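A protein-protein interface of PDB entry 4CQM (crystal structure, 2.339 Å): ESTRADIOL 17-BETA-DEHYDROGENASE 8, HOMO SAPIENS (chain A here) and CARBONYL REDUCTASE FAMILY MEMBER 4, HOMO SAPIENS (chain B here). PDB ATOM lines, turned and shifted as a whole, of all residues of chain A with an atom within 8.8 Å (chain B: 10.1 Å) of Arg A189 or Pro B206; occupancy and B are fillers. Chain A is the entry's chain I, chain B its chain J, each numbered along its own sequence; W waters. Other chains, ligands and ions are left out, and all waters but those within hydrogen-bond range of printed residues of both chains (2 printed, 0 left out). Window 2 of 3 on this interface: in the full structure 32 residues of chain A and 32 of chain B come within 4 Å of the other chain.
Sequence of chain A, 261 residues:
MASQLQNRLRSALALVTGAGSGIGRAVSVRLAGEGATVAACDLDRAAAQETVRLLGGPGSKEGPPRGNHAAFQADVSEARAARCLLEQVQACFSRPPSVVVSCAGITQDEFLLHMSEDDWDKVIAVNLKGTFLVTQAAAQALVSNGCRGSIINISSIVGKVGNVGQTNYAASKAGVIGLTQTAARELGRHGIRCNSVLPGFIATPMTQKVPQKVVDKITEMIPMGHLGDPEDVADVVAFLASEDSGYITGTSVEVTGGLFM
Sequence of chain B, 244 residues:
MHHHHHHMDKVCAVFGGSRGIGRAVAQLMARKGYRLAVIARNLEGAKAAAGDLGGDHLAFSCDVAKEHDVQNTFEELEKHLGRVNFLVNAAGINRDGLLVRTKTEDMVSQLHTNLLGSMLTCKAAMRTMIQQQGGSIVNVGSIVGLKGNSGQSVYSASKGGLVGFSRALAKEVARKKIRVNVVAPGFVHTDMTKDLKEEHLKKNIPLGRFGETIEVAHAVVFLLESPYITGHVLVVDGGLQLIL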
ATOM      1  N   VAL A 143     -10.293   0.251   0.318  1.00  0.00           N
ATOM      2  CA  VAL A 143      -9.573  -0.072  -0.908  1.00  0.00           C
ATOM      3  C   VAL A 143     -10.546  -0.455  -2.022  1.00  0.00           C
ATOM      4  O   VAL A 143     -10.348  -0.101  -3.185  1.00  0.00           O
ATOM      5  CB  VAL A 143      -8.564  -1.221  -0.685  1.00  0.00           C
ATOM      6  CG1 VAL A 143      -7.863  -1.583  -1.985  1.00  0.00           C
ATOM      7  CG2 VAL A 143      -7.546  -0.833   0.375  1.00  0.00           C
ATOM      8  N   ARG A 148     -10.078   7.447   0.331  1.00  0.00           N
ATOM      9  CA  ARG A 148      -9.005   7.736   1.272  1.00  0.00           C
ATOM     10  C   ARG A 148      -9.540   7.599   2.692  1.00  0.00           C
ATOM     11  O   ARG A 148     -10.751   7.622   2.908  1.00  0.00           O
ATOM     12  CB  ARG A 148      -8.437   9.137   1.039  1.00  0.00           C
ATOM     13  CG  ARG A 148      -7.915   9.368  -0.371  1.00  0.00           C
ATOM     14  CD  ARG A 148      -7.408  10.791  -0.552  1.00  0.00           C
ATOM     15  NE  ARG A 148      -6.275  11.085   0.320  1.00  0.00           N
ATOM     16  N   GLN A 181       2.062   0.426  12.524  1.00  0.00           N
ATOM     17  CA  GLN A 181       3.229   0.804  11.733  1.00  0.00           C
ATOM     18  C   GLN A 181       3.291   0.016  10.429  1.00  0.00           C
ATOM     19  O   GLN A 181       3.691   0.545   9.392  1.00  0.00           O
ATOM     20  CB  GLN A 181       4.512   0.590  12.536  1.00  0.00           C
ATOM     21  CG  GLN A 181       4.739   1.616  13.634  1.00  0.00           C
ATOM     22  CD  GLN A 181       5.864   1.225  14.572  1.00  0.00           C
ATOM     23  OE1 GLN A 181       6.119   0.041  14.793  1.00  0.00           O
ATOM     24  NE2 GLN A 181       6.546   2.220  15.125  1.00  0.00           N
ATOM     25  N   THR A 182       2.893  -1.250  10.488  1.00  0.00           N
ATOM     26  CA  THR A 182       2.871  -2.097   9.302  1.00  0.00           C
ATOM     27  C   THR A 182       1.729  -1.692   8.376  1.00  0.00           C
ATOM     28  O   THR A 182       1.907  -1.591   7.162  1.00  0.00           O
ATOM     29  CB  THR A 182       2.727  -3.585   9.670  1.00  0.00           C
ATOM     30  OG1 THR A 182       3.863  -4.004  10.437  1.00  0.00           O
ATOM     31  CG2 THR A 182       2.633  -4.435   8.415  1.00  0.00           C
ATOM     32  N   ALA A 183       0.559  -1.459   8.963  1.00  0.00           N
ATOM     33  CA  ALA A 183      -0.621  -1.059   8.205  1.00  0.00           C
ATOM     34  C   ALA A 183      -0.377   0.247   7.459  1.00  0.00           C
ATOM     35  O   ALA A 183      -0.776   0.399   6.306  1.00  0.00           O
ATOM     36  CB  ALA A 183      -1.823  -0.925   9.128  1.00  0.00           C
ATOM     37  N   ALA A 184       0.290   1.184   8.125  1.00  0.00           N
ATOM     38  CA  ALA A 184       0.605   2.476   7.530  1.00  0.00           C
ATOM     39  C   ALA A 184       1.533   2.326   6.330  1.00  0.00           C
ATOM     40  O   ALA A 184       1.454   3.095   5.372  1.00  0.00           O
ATOM     41  CB  ALA A 184       1.231   3.390   8.567  1.00  0.00           C
ATOM     42  N   ARG A 185       2.408   1.328   6.389  1.00  0.00           N
ATOM     43  CA  ARG A 185       3.403   1.110   5.346  1.00  0.00           C
ATOM     44  C   ARG A 185       2.778   0.481   4.104  1.00  0.00           C
ATOM     45  O   ARG A 185       3.216   0.735   2.982  1.00  0.00           O
ATOM     46  CB  ARG A 185       4.538   0.229   5.876  1.00  0.00           C
ATOM     47  CG  ARG A 185       5.862   0.387   5.141  1.00  0.00           C
ATOM     48  CD  ARG A 185       6.071  -0.701   4.099  1.00  0.00           C
ATOM     49  NE  ARG A 185       7.349  -0.550   3.409  1.00  0.00           N
ATOM     50  CZ  ARG A 185       8.502  -1.049   3.847  1.00  0.00           C
ATOM     51  NH1 ARG A 185       8.541  -1.735   4.981  1.00  0.00           N
ATOM     52  NH2 ARG A 185       9.615  -0.861   3.153  1.00  0.00           N
ATOM     53  N   GLU A 186       1.750  -0.336   4.310  1.00  0.00           N
ATOM     54  CA  GLU A 186       1.083  -1.014   3.203  1.00  0.00           C
ATOM     55  C   GLU A 186      -0.026  -0.158   2.599  1.00  0.00           C
ATOM     56  O   GLU A 186      -0.218  -0.141   1.382  1.00  0.00           O
ATOM     57  CB  GLU A 186       0.510  -2.356   3.665  1.00  0.00           C
ATOM     58  CG  GLU A 186       1.557  -3.346   4.150  1.00  0.00           C
ATOM     59  CD  GLU A 186       0.963  -4.697   4.499  1.00  0.00           C
ATOM     60  OE1 GLU A 186      -0.252  -4.888   4.283  1.00  0.00           O
ATOM     61  OE2 GLU A 186       1.712  -5.569   4.988  1.00  0.00           O
ATOM     62  N   LEU A 187      -0.753   0.554   3.454  1.00  0.00           N
ATOM     63  CA  LEU A 187      -1.889   1.356   3.012  1.00  0.00           C
ATOM     64  C   LEU A 187      -1.473   2.768   2.615  1.00  0.00           C
ATOM     65  O   LEU A 187      -2.317   3.601   2.282  1.00  0.00           O
ATOM     66  CB  LEU A 187      -2.952   1.417   4.109  1.00  0.00           C
ATOM     67  CG  LEU A 187      -3.494   0.075   4.604  1.00  0.00           C
ATOM     68  CD1 LEU A 187      -4.470   0.288   5.749  1.00  0.00           C
ATOM     69  CD2 LEU A 187      -4.150  -0.700   3.470  1.00  0.00           C
ATOM     70  N   GLY A 188      -0.170   3.032   2.654  1.00  0.00           N
ATOM     71  CA  GLY A 188       0.357   4.343   2.324  1.00  0.00           C
ATOM     72  C   GLY A 188       0.033   4.773   0.906  1.00  0.00           C
ATOM     73  O   GLY A 188      -0.503   5.860   0.687  1.00  0.00           O
ATOM     74  N   ARG A 189       0.352   3.917  -0.060  1.00  0.00           N
ATOM     75  CA  ARG A 189       0.090   4.221  -1.463  1.00  0.00           C
ATOM     76  C   ARG A 189      -1.352   3.900  -1.851  1.00  0.00           C
ATOM     77  O   ARG A 189      -1.700   3.897  -3.032  1.00  0.00           O
ATOM     78  CB  ARG A 189       1.072   3.466  -2.367  1.00  0.00           C
ATOM     79  CG  ARG A 189       1.401   2.047  -1.921  1.00  0.00           C
ATOM     80  CD  ARG A 189       0.364   1.044  -2.395  1.00  0.00           C
ATOM     81  NE  ARG A 189       0.701  -0.319  -1.994  1.00  0.00           N
ATOM     82  N   HIS A 190      -2.185   3.630  -0.851  1.00  0.00           N
ATOM     83  CA  HIS A 190      -3.614   3.447  -1.067  1.00  0.00           C
ATOM     84  C   HIS A 190      -4.394   4.614  -0.475  1.00  0.00           C
ATOM     85  O   HIS A 190      -5.619   4.570  -0.372  1.00  0.00           O
ATOM     86  CB  HIS A 190      -4.095   2.125  -0.464  1.00  0.00           C
ATOM     87  CG  HIS A 190      -3.762   0.926  -1.295  1.00  0.00           C
ATOM     88  ND1 HIS A 190      -2.610   0.191  -1.116  1.00  0.00           N
ATOM     89  CD2 HIS A 190      -4.429   0.336  -2.316  1.00  0.00           C
ATOM     90  CE1 HIS A 190      -2.584  -0.802  -1.988  1.00  0.00           C
ATOM     91  NE2 HIS A 190      -3.676  -0.736  -2.728  1.00  0.00           N
ATOM     92  N   GLY A 191      -3.669   5.658  -0.085  1.00  0.00           N
ATOM     93  CA  GLY A 191      -4.278   6.863   0.444  1.00  0.00           C
ATOM     94  C   GLY A 191      -4.908   6.681   1.811  1.00  0.00           C
ATOM     95  O   GLY A 191      -5.884   7.352   2.146  1.00  0.00           O
ATOM     96  N   ILE A 192      -4.350   5.773   2.606  1.00  0.00           N
ATOM     97  CA  ILE A 192      -4.870   5.515   3.944  1.00  0.00           C
ATOM     98  C   ILE A 192      -3.793   5.684   5.010  1.00  0.00           C
ATOM     99  O   ILE A 192      -2.783   4.980   5.004  1.00  0.00           O
ATOM    100  CB  ILE A 192      -5.463   4.100   4.057  1.00  0.00           C
ATOM    101  CG1 ILE A 192      -6.573   3.902   3.024  1.00  0.00           C
ATOM    102  CG2 ILE A 192      -5.989   3.855   5.462  1.00  0.00           C
ATOM    103  CD1 ILE A 192      -7.151   2.507   3.014  1.00  0.00           C
ATOM    104  N   ARG A 193      -4.017   6.622   5.924  1.00  0.00           N
ATOM    105  CA  ARG A 193      -3.081   6.876   7.013  1.00  0.00           C
ATOM    106  C   ARG A 193      -3.400   6.004   8.222  1.00  0.00           C
ATOM    107  O   ARG A 193      -4.562   5.702   8.492  1.00  0.00           O
ATOM    108  CB  ARG A 193      -3.103   8.356   7.406  1.00  0.00           C
ATOM    109  CG  ARG A 193      -2.606   9.294   6.315  1.00  0.00           C
ATOM    110  CD  ARG A 193      -2.615  10.752   6.762  1.00  0.00           C
ATOM    111  NE  ARG A 193      -3.967  11.292   6.891  1.00  0.00           N
ATOM    112  CZ  ARG A 193      -4.573  11.529   8.050  1.00  0.00           C
ATOM    113  NH1 ARG A 193      -3.947  11.277   9.192  1.00  0.00           N
ATOM    114  NH2 ARG A 193      -5.804  12.022   8.068  1.00  0.00           N
ATOM    115  N   CYS A 194      -2.360   5.596   8.942  1.00  0.00           N
ATOM    116  CA  CYS A 194      -2.529   4.786  10.143  1.00  0.00           C
ATOM    117  C   CYS A 194      -1.666   5.319  11.278  1.00  0.00           C
ATOM    118  O   CYS A 194      -0.451   5.458  11.133  1.00  0.00           O
ATOM    119  CB  CYS A 194      -2.185   3.321   9.862  1.00  0.00           C
ATOM    120  SG  CYS A 194      -3.232   2.528   8.622  1.00  0.00           S
ATOM    121  N   TYR A 247      -0.069  14.511   6.478  1.00  0.00           N
ATOM    122  CA  TYR A 247       1.269  13.982   6.244  1.00  0.00           C
ATOM    123  C   TYR A 247       1.760  13.201   7.460  1.00  0.00           C
ATOM    124  O   TYR A 247       2.961  12.999   7.641  1.00  0.00           O
ATOM    125  CB  TYR A 247       2.239  15.115   5.902  1.00  0.00           C
ATOM    126  CG  TYR A 247       3.503  14.659   5.205  1.00  0.00           C
ATOM    127  CD1 TYR A 247       3.445  13.998   3.985  1.00  0.00           C
ATOM    128  CD2 TYR A 247       4.752  14.901   5.759  1.00  0.00           C
ATOM    129  CE1 TYR A 247       4.596  13.580   3.342  1.00  0.00           C
ATOM    130  CE2 TYR A 247       5.909  14.489   5.123  1.00  0.00           C
ATOM    131  CZ  TYR A 247       5.824  13.830   3.916  1.00  0.00           C
ATOM    132  OH  TYR A 247       6.974  13.418   3.280  1.00  0.00           O
ATOM    133  N   ILE A 248       0.819  12.759   8.289  1.00  0.00           N
ATOM    134  CA  ILE A 248       1.150  12.000   9.490  1.00  0.00           C
ATOM    135  C   ILE A 248       0.607  10.576   9.422  1.00  0.00           C
ATOM    136  O   ILE A 248      -0.602  10.356   9.501  1.00  0.00           O
ATOM    137  CB  ILE A 248       0.599  12.683  10.757  1.00  0.00           C
ATOM    138  CG1 ILE A 248       1.182  14.089  10.903  1.00  0.00           C
ATOM    139  CG2 ILE A 248       0.906  11.848  11.991  1.00  0.00           C
ATOM    140  CD1 ILE A 248       0.766  14.795  12.176  1.00  0.00           C
ATOM    141  N   THR A 249       1.509   9.611   9.270  1.00  0.00           N
ATOM    142  CA  THR A 249       1.130   8.204   9.268  1.00  0.00           C
ATOM    143  C   THR A 249       2.239   7.364   9.896  1.00  0.00           C
ATOM    144  O   THR A 249       3.410   7.742   9.862  1.00  0.00           O
ATOM    145  CB  THR A 249       0.828   7.694   7.843  1.00  0.00           C
ATOM    146  OG1 THR A 249       0.292   6.367   7.909  1.00  0.00           O
ATOM    147  CG2 THR A 249       2.084   7.691   6.986  1.00  0.00           C
ATOM    148  N   GLY A 250       1.861   6.228  10.476  1.00  0.00           N
ATOM    149  CA  GLY A 250       2.808   5.376  11.174  1.00  0.00           C
ATOM    150  C   GLY A 250       3.426   6.093  12.358  1.00  0.00           C
ATOM    151  O   GLY A 250       4.593   5.881  12.688  1.00  0.00           O
ATOM    152  N   PHE B 187      10.806  15.267   5.274  1.00  0.00           N
ATOM    153  CA  PHE B 187      11.255  16.085   4.155  1.00  0.00           C
ATOM    154  C   PHE B 187      10.182  17.097   3.767  1.00  0.00           C
ATOM    155  O   PHE B 187       9.115  16.729   3.276  1.00  0.00           O
ATOM    156  CB  PHE B 187      11.621  15.201   2.963  1.00  0.00           C
ATOM    157  CG  PHE B 187      12.829  14.339   3.202  1.00  0.00           C
ATOM    158  CD1 PHE B 187      13.947  14.854   3.836  1.00  0.00           C
ATOM    159  CD2 PHE B 187      12.840  13.012   2.805  1.00  0.00           C
ATOM    160  CE1 PHE B 187      15.059  14.065   4.062  1.00  0.00           C
ATOM    161  CE2 PHE B 187      13.949  12.217   3.029  1.00  0.00           C
ATOM    162  CZ  PHE B 187      15.059  12.745   3.659  1.00  0.00           C
ATOM    163  N   LEU B 201      14.073   9.466  -3.667  1.00  0.00           N
ATOM    164  CA  LEU B 201      13.749   9.335  -2.250  1.00  0.00           C
ATOM    165  C   LEU B 201      12.306   8.907  -2.017  1.00  0.00           C
ATOM    166  O   LEU B 201      12.043   7.935  -1.307  1.00  0.00           O
ATOM    167  CB  LEU B 201      14.010  10.654  -1.521  1.00  0.00           C
ATOM    168  CG  LEU B 201      15.380  10.856  -0.866  1.00  0.00           C
ATOM    169  CD1 LEU B 201      16.515  10.672  -1.864  1.00  0.00           C
ATOM    170  CD2 LEU B 201      15.453  12.229  -0.215  1.00  0.00           C
ATOM    171  N   LYS B 202      11.375   9.639  -2.624  1.00  0.00           N
ATOM    172  CA  LYS B 202       9.948   9.459  -2.366  1.00  0.00           C
ATOM    173  C   LYS B 202       9.407   8.115  -2.845  1.00  0.00           C
ATOM    174  O   LYS B 202       8.263   7.766  -2.555  1.00  0.00           O
ATOM    175  CB  LYS B 202       9.150  10.591  -3.017  1.00  0.00           C
ATOM    176  N   LYS B 203      10.223   7.364  -3.579  1.00  0.00           N
ATOM    177  CA  LYS B 203       9.830   6.031  -4.018  1.00  0.00           C
ATOM    178  C   LYS B 203       9.704   5.099  -2.817  1.00  0.00           C
ATOM    179  O   LYS B 203       8.983   4.103  -2.862  1.00  0.00           O
ATOM    180  CB  LYS B 203      10.838   5.471  -5.024  1.00  0.00           C
ATOM    181  N   ASN B 204      10.411   5.438  -1.743  1.00  0.00           N
ATOM    182  CA  ASN B 204      10.364   4.659  -0.513  1.00  0.00           C
ATOM    183  C   ASN B 204       9.278   5.153   0.437  1.00  0.00           C
ATOM    184  O   ASN B 204       8.524   4.353   0.991  1.00  0.00           O
ATOM    185  CB  ASN B 204      11.724   4.693   0.184  1.00  0.00           C
ATOM    186  CG  ASN B 204      12.827   4.079  -0.657  1.00  0.00           C
ATOM    187  OD1 ASN B 204      12.613   3.726  -1.817  1.00  0.00           O
ATOM    188  ND2 ASN B 204      14.014   3.952  -0.076  1.00  0.00           N
ATOM    189  N   ILE B 205       9.206   6.472   0.611  1.00  0.00           N
ATOM    190  CA  ILE B 205       8.243   7.107   1.514  1.00  0.00           C
ATOM    191  C   ILE B 205       6.812   6.620   1.282  1.00  0.00           C
ATOM    192  O   ILE B 205       6.317   6.659   0.156  1.00  0.00           O
ATOM    193  CB  ILE B 205       8.282   8.645   1.367  1.00  0.00           C
ATOM    194  CG1 ILE B 205       9.668   9.179   1.736  1.00  0.00           C
ATOM    195  CG2 ILE B 205       7.211   9.301   2.227  1.00  0.00           C
ATOM    196  CD1 ILE B 205       9.775  10.689   1.688  1.00  0.00           C
ATOM    197  N   PRO B 206       6.154   6.146   2.355  1.00  0.00           N
ATOM    198  CA  PRO B 206       4.803   5.570   2.320  1.00  0.00           C
ATOM    199  C   PRO B 206       3.768   6.456   1.631  1.00  0.00           C
ATOM    200  O   PRO B 206       2.935   5.944   0.883  1.00  0.00           O
ATOM    201  CB  PRO B 206       4.462   5.401   3.802  1.00  0.00           C
ATOM    202  CG  PRO B 206       5.777   5.201   4.455  1.00  0.00           C
ATOM    203  CD  PRO B 206       6.736   6.085   3.708  1.00  0.00           C
ATOM    204  N   LEU B 207       3.819   7.761   1.879  1.00  0.00           N
ATOM    205  CA  LEU B 207       2.877   8.683   1.256  1.00  0.00           C
ATOM    206  C   LEU B 207       3.355   9.114  -0.129  1.00  0.00           C
ATOM    207  O   LEU B 207       2.642   9.810  -0.853  1.00  0.00           O
ATOM    208  CB  LEU B 207       2.649   9.904   2.148  1.00  0.00           C
ATOM    209  CG  LEU B 207       1.904   9.625   3.456  1.00  0.00           C
ATOM    210  CD1 LEU B 207       1.530  10.922   4.152  1.00  0.00           C
ATOM    211  CD2 LEU B 207       0.667   8.775   3.203  1.00  0.00           C
ATOM    212  N   GLY B 208       4.565   8.696  -0.487  1.00  0.00           N
ATOM    213  CA  GLY B 208       5.094   8.904  -1.824  1.00  0.00           C
ATOM    214  C   GLY B 208       5.367  10.346  -2.207  1.00  0.00           C
ATOM    215  O   GLY B 208       5.520  10.660  -3.387  1.00  0.00           O
ATOM    216  N   ARG B 209       5.434  11.226  -1.214  1.00  0.00           N
ATOM    217  CA  ARG B 209       5.662  12.641  -1.477  1.00  0.00           C
ATOM    218  C   ARG B 209       6.346  13.334  -0.307  1.00  0.00           C
ATOM    219  O   ARG B 209       6.482  12.763   0.776  1.00  0.00           O
ATOM    220  CB  ARG B 209       4.338  13.345  -1.783  1.00  0.00           C
ATOM    221  CG  ARG B 209       3.363  13.346  -0.615  1.00  0.00           C
ATOM    222  CD  ARG B 209       2.146  14.208  -0.899  1.00  0.00           C
ATOM    223  NE  ARG B 209       1.210  14.209   0.222  1.00  0.00           N
ATOM    224  CZ  ARG B 209       1.266  15.058   1.243  1.00  0.00           C
ATOM    225  NH1 ARG B 209       2.217  15.981   1.289  1.00  0.00           N
ATOM    226  NH2 ARG B 209       0.371  14.985   2.220  1.00  0.00           N
ATOM    227  N   PHE B 210       6.779  14.570  -0.535  1.00  0.00           N
ATOM    228  CA  PHE B 210       7.295  15.407   0.540  1.00  0.00           C
ATOM    229  C   PHE B 210       6.146  16.163   1.189  1.00  0.00           C
ATOM    230  O   PHE B 210       5.071  16.297   0.604  1.00  0.00           O
ATOM    231  CB  PHE B 210       8.348  16.390   0.023  1.00  0.00           C
ATOM    232  CG  PHE B 210       9.697  15.772  -0.218  1.00  0.00           C
ATOM    233  CD1 PHE B 210       9.885  14.405  -0.098  1.00  0.00           C
ATOM    234  CD2 PHE B 210      10.783  16.567  -0.550  1.00  0.00           C
ATOM    235  CE1 PHE B 210      11.127  13.840  -0.317  1.00  0.00           C
ATOM    236  CE2 PHE B 210      12.028  16.007  -0.767  1.00  0.00           C
ATOM    237  CZ  PHE B 210      12.200  14.643  -0.651  1.00  0.00           C
ATOM    238  N   VAL B 236       6.158  14.106  11.835  1.00  0.00           N
ATOM    239  CA  VAL B 236       5.427  14.440  10.617  1.00  0.00           C
ATOM    240  C   VAL B 236       6.305  14.196   9.392  1.00  0.00           C
ATOM    241  O   VAL B 236       6.860  15.132   8.819  1.00  0.00           O
ATOM    242  CB  VAL B 236       4.955  15.906  10.622  1.00  0.00           C
ATOM    243  CG1 VAL B 236       3.920  16.138   9.528  1.00  0.00           C
ATOM    244  CG2 VAL B 236       4.381  16.274  11.979  1.00  0.00           C
ATOM    245  N   ASP B 237       6.426  12.936   8.990  1.00  0.00           N
ATOM    246  CA  ASP B 237       7.346  12.569   7.920  1.00  0.00           C
ATOM    247  C   ASP B 237       6.678  11.740   6.829  1.00  0.00           C
ATOM    248  O   ASP B 237       7.323  11.344   5.859  1.00  0.00           O
ATOM    249  CB  ASP B 237       8.534  11.800   8.497  1.00  0.00           C
ATOM    250  CG  ASP B 237       8.114  10.524   9.199  1.00  0.00           C
ATOM    251  OD1 ASP B 237       6.924  10.409   9.562  1.00  0.00           O
ATOM    252  OD2 ASP B 237       8.974   9.640   9.394  1.00  0.00           O
ATOM    253  N   GLY B 238       5.386  11.478   6.994  1.00  0.00           N
ATOM    254  CA  GLY B 238       4.651  10.680   6.032  1.00  0.00           C
ATOM    255  C   GLY B 238       5.025   9.212   6.090  1.00  0.00           C
ATOM    256  O   GLY B 238       4.824   8.471   5.127  1.00  0.00           O
ATOM    257  N   GLY B 239       5.574   8.789   7.225  1.00  0.00           N
ATOM    258  CA  GLY B 239       5.947   7.401   7.426  1.00  0.00           C
ATOM    259  C   GLY B 239       7.390   7.103   7.070  1.00  0.00           C
ATOM    260  O   GLY B 239       7.766   5.946   6.878  1.00  0.00           O
ATOM    261  N   LEU B 240       8.204   8.151   6.988  1.00  0.00           N
ATOM    262  CA  LEU B 240       9.609   8.008   6.621  1.00  0.00           C
ATOM    263  C   LEU B 240      10.415   7.278   7.695  1.00  0.00           C
ATOM    264  O   LEU B 240      11.367   6.559   7.385  1.00  0.00           O
ATOM    265  CB  LEU B 240      10.223   9.386   6.354  1.00  0.00           C
ATOM    266  CG  LEU B 240      11.709   9.432   5.992  1.00  0.00           C
ATOM    267  CD1 LEU B 240      11.970   8.670   4.702  1.00  0.00           C
ATOM    268  CD2 LEU B 240      12.187  10.872   5.876  1.00  0.00           C
ATOM    269  N   GLN B 241      10.024   7.455   8.953  1.00  0.00           N
ATOM    270  CA  GLN B 241      10.764   6.891  10.080  1.00  0.00           C
ATOM    271  C   GLN B 241      10.729   5.364  10.114  1.00  0.00           C
ATOM    272  O   GLN B 241      11.499   4.737  10.840  1.00  0.00           O
ATOM    273  CB  GLN B 241      10.222   7.440  11.400  1.00  0.00           C
ATOM    274  CG  GLN B 241       8.760   7.116  11.649  1.00  0.00           C
ATOM    275  CD  GLN B 241       8.310   7.505  13.042  1.00  0.00           C
ATOM    276  OE1 GLN B 241       9.131   7.713  13.936  1.00  0.00           O
ATOM    277  NE2 GLN B 241       7.000   7.606  13.235  1.00  0.00           N
ATOM    278  N   LEU B 242       9.832   4.772   9.334  1.00  0.00           N
ATOM    279  CA  LEU B 242       9.711   3.320   9.278  1.00  0.00           C
ATOM    280  C   LEU B 242      10.695   2.729   8.273  1.00  0.00           C
ATOM    281  O   LEU B 242      10.750   1.515   8.082  1.00  0.00           O
ATOM    282  CB  LEU B 242       8.280   2.917   8.916  1.00  0.00           C
ATOM    283  CG  LEU B 242       7.169   3.536   9.766  1.00  0.00           C
ATOM    284  CD1 LEU B 242       5.800   3.103   9.262  1.00  0.00           C
ATOM    285  CD2 LEU B 242       7.342   3.176  11.235  1.00  0.00           C
ATOM    286  N   ILE B 243      11.467   3.602   7.631  1.00  0.00           N
ATOM    287  CA  ILE B 243      12.407   3.196   6.591  1.00  0.00           C
ATOM    288  C   ILE B 243      13.791   3.777   6.865  1.00  0.00           C
ATOM    289  O   ILE B 243      14.810   3.201   6.483  1.00  0.00           O
ATOM    290  CB  ILE B 243      11.927   3.650   5.195  1.00  0.00           C
ATOM    291  CG1 ILE B 243      10.472   3.238   4.972  1.00  0.00           C
ATOM    292  CG2 ILE B 243      12.816   3.081   4.099  1.00  0.00           C
ATOM    293  CD1 ILE B 243       9.838   3.892   3.779  1.00  0.00           C
ATOM    294  N   LEU B 244      13.812   4.918   7.545  1.00  0.00           N
ATOM    295  CA  LEU B 244      15.048   5.645   7.815  1.00  0.00           C
ATOM    296  C   LEU B 244      16.008   4.850   8.697  1.00  0.00           C
ATOM    297  O   LEU B 244      15.638   3.832   9.281  1.00  0.00           O
ATOM    298  CB  LEU B 244      14.730   6.989   8.469  1.00  0.00           C
ATOM    299  CG  LEU B 244      15.558   8.187   8.004  1.00  0.00           C
ATOM    300  CD1 LEU B 244      15.422   8.372   6.501  1.00  0.00           C
ATOM    301  CD2 LEU B 244      15.133   9.446   8.742  1.00  0.00           C
HETATM  302  O   HOH W   1       4.352  11.015   9.980  1.00  0.00           O
HETATM  303  O   HOH W   2       9.364  12.642   4.805  1.00  0.00           O
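The backbone carbonyl oxygen of Pro B206 sits at hydrogen-bond distance from the backbone NH of Arg A189 (3.4 Å).
OH of Tyr A247 is in hydrogen-bond range of O of Arg B209, 2.6 Å away.
OH of Tyr A247 sits at hydrogen-bond distance from O of Asp B237 (3.3 Å).
The backbone NH (N) of Gly B238 lies within hydrogen-bond range of the backbone carbonyl oxygen (O) of Tyr A247.
The side-chain amide nitrogen (NE2) of Gln B241 lies within hydrogen-bond range of the backbone carbonyl oxygen (O) of Gly A250 (3.0 Å).
The backbone carbonyl oxygen of Gly A188 lies close to the backbone carbonyl oxygen of Pro B206 (3.4 Å).
The guanidinium group (NE) of Arg A189 sits close to a ring nitrogen (ND1) of His A190.
The side-chain carboxylate (OD2) of Asp B237 is in hydrogen-bond range of the backbone NH (N) of Gln B241 (2.5 Å).
Among the printed residues, merely in contact across the chains: Gln A181 with Leu B242 (3.3 Å), Tyr A247 with Phe B187 (3.9 Å), Tyr A247 with Leu B207 (3.6 Å), Tyr A247 with Phe B210 (3.4 Å), Tyr A247 with Val B236 (3.7 Å), Ile A248 with Val B236 (3.7 Å), Thr A249 with Gly B238 (3.4 Å) and Thr A249 with Gly B239 (3.5 Å).
Gly A188 touches just one residue of chain B: Pro B206 (3.1 Å).
Printed residues of chain A within 4 Å of Phe B187: Tyr A247 (3.9 Å).
Of the printed residues of chain B, Tyr A247 touches Phe B187 (3.9 Å), Leu B207 (3.6 Å), Arg B209 (2.6 Å), Phe B210 (3.4 Å), Val B236 (3.7 Å), Asp B237 (3.3 Å) and Gly B238 (2.9 Å).
The nearest residue of chain B that does not touch Arg A189 is Leu B207 (5.5 Å).
The nearest residue of chain A that does not touch Pro B206 is Ala A184 (4.1 Å).
The nearest printed residue of chain A that does not touch Gln B241 is Thr A249 (4.9 Å).
Printed residues of chain B that touch a printed residue of chain A: Phe B187, Pro B206, Leu B207, Arg B209, Phe B210, Val B236, Asp B237, Gly B238, Gly B239, Gln B241 and Leu B242.
Hydrophobic or aromatic side chains of chain A that line the printed part of chain B: Tyr A247 and Ile A248.
Along chain A the printed residues that touch a printed residue of chain B span positions 181 to 250.
Among the printed residues, 14 pairs touch across the chains.
Among the printed residues, no Asp or Glu carboxylate lies within 4 Å of a Lys or Arg side-chain nitrogen of the other chain.
Water W2 lies within hydrogen-bond range of O of Asp B237, OH of Tyr A247 and N of Phe B187.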
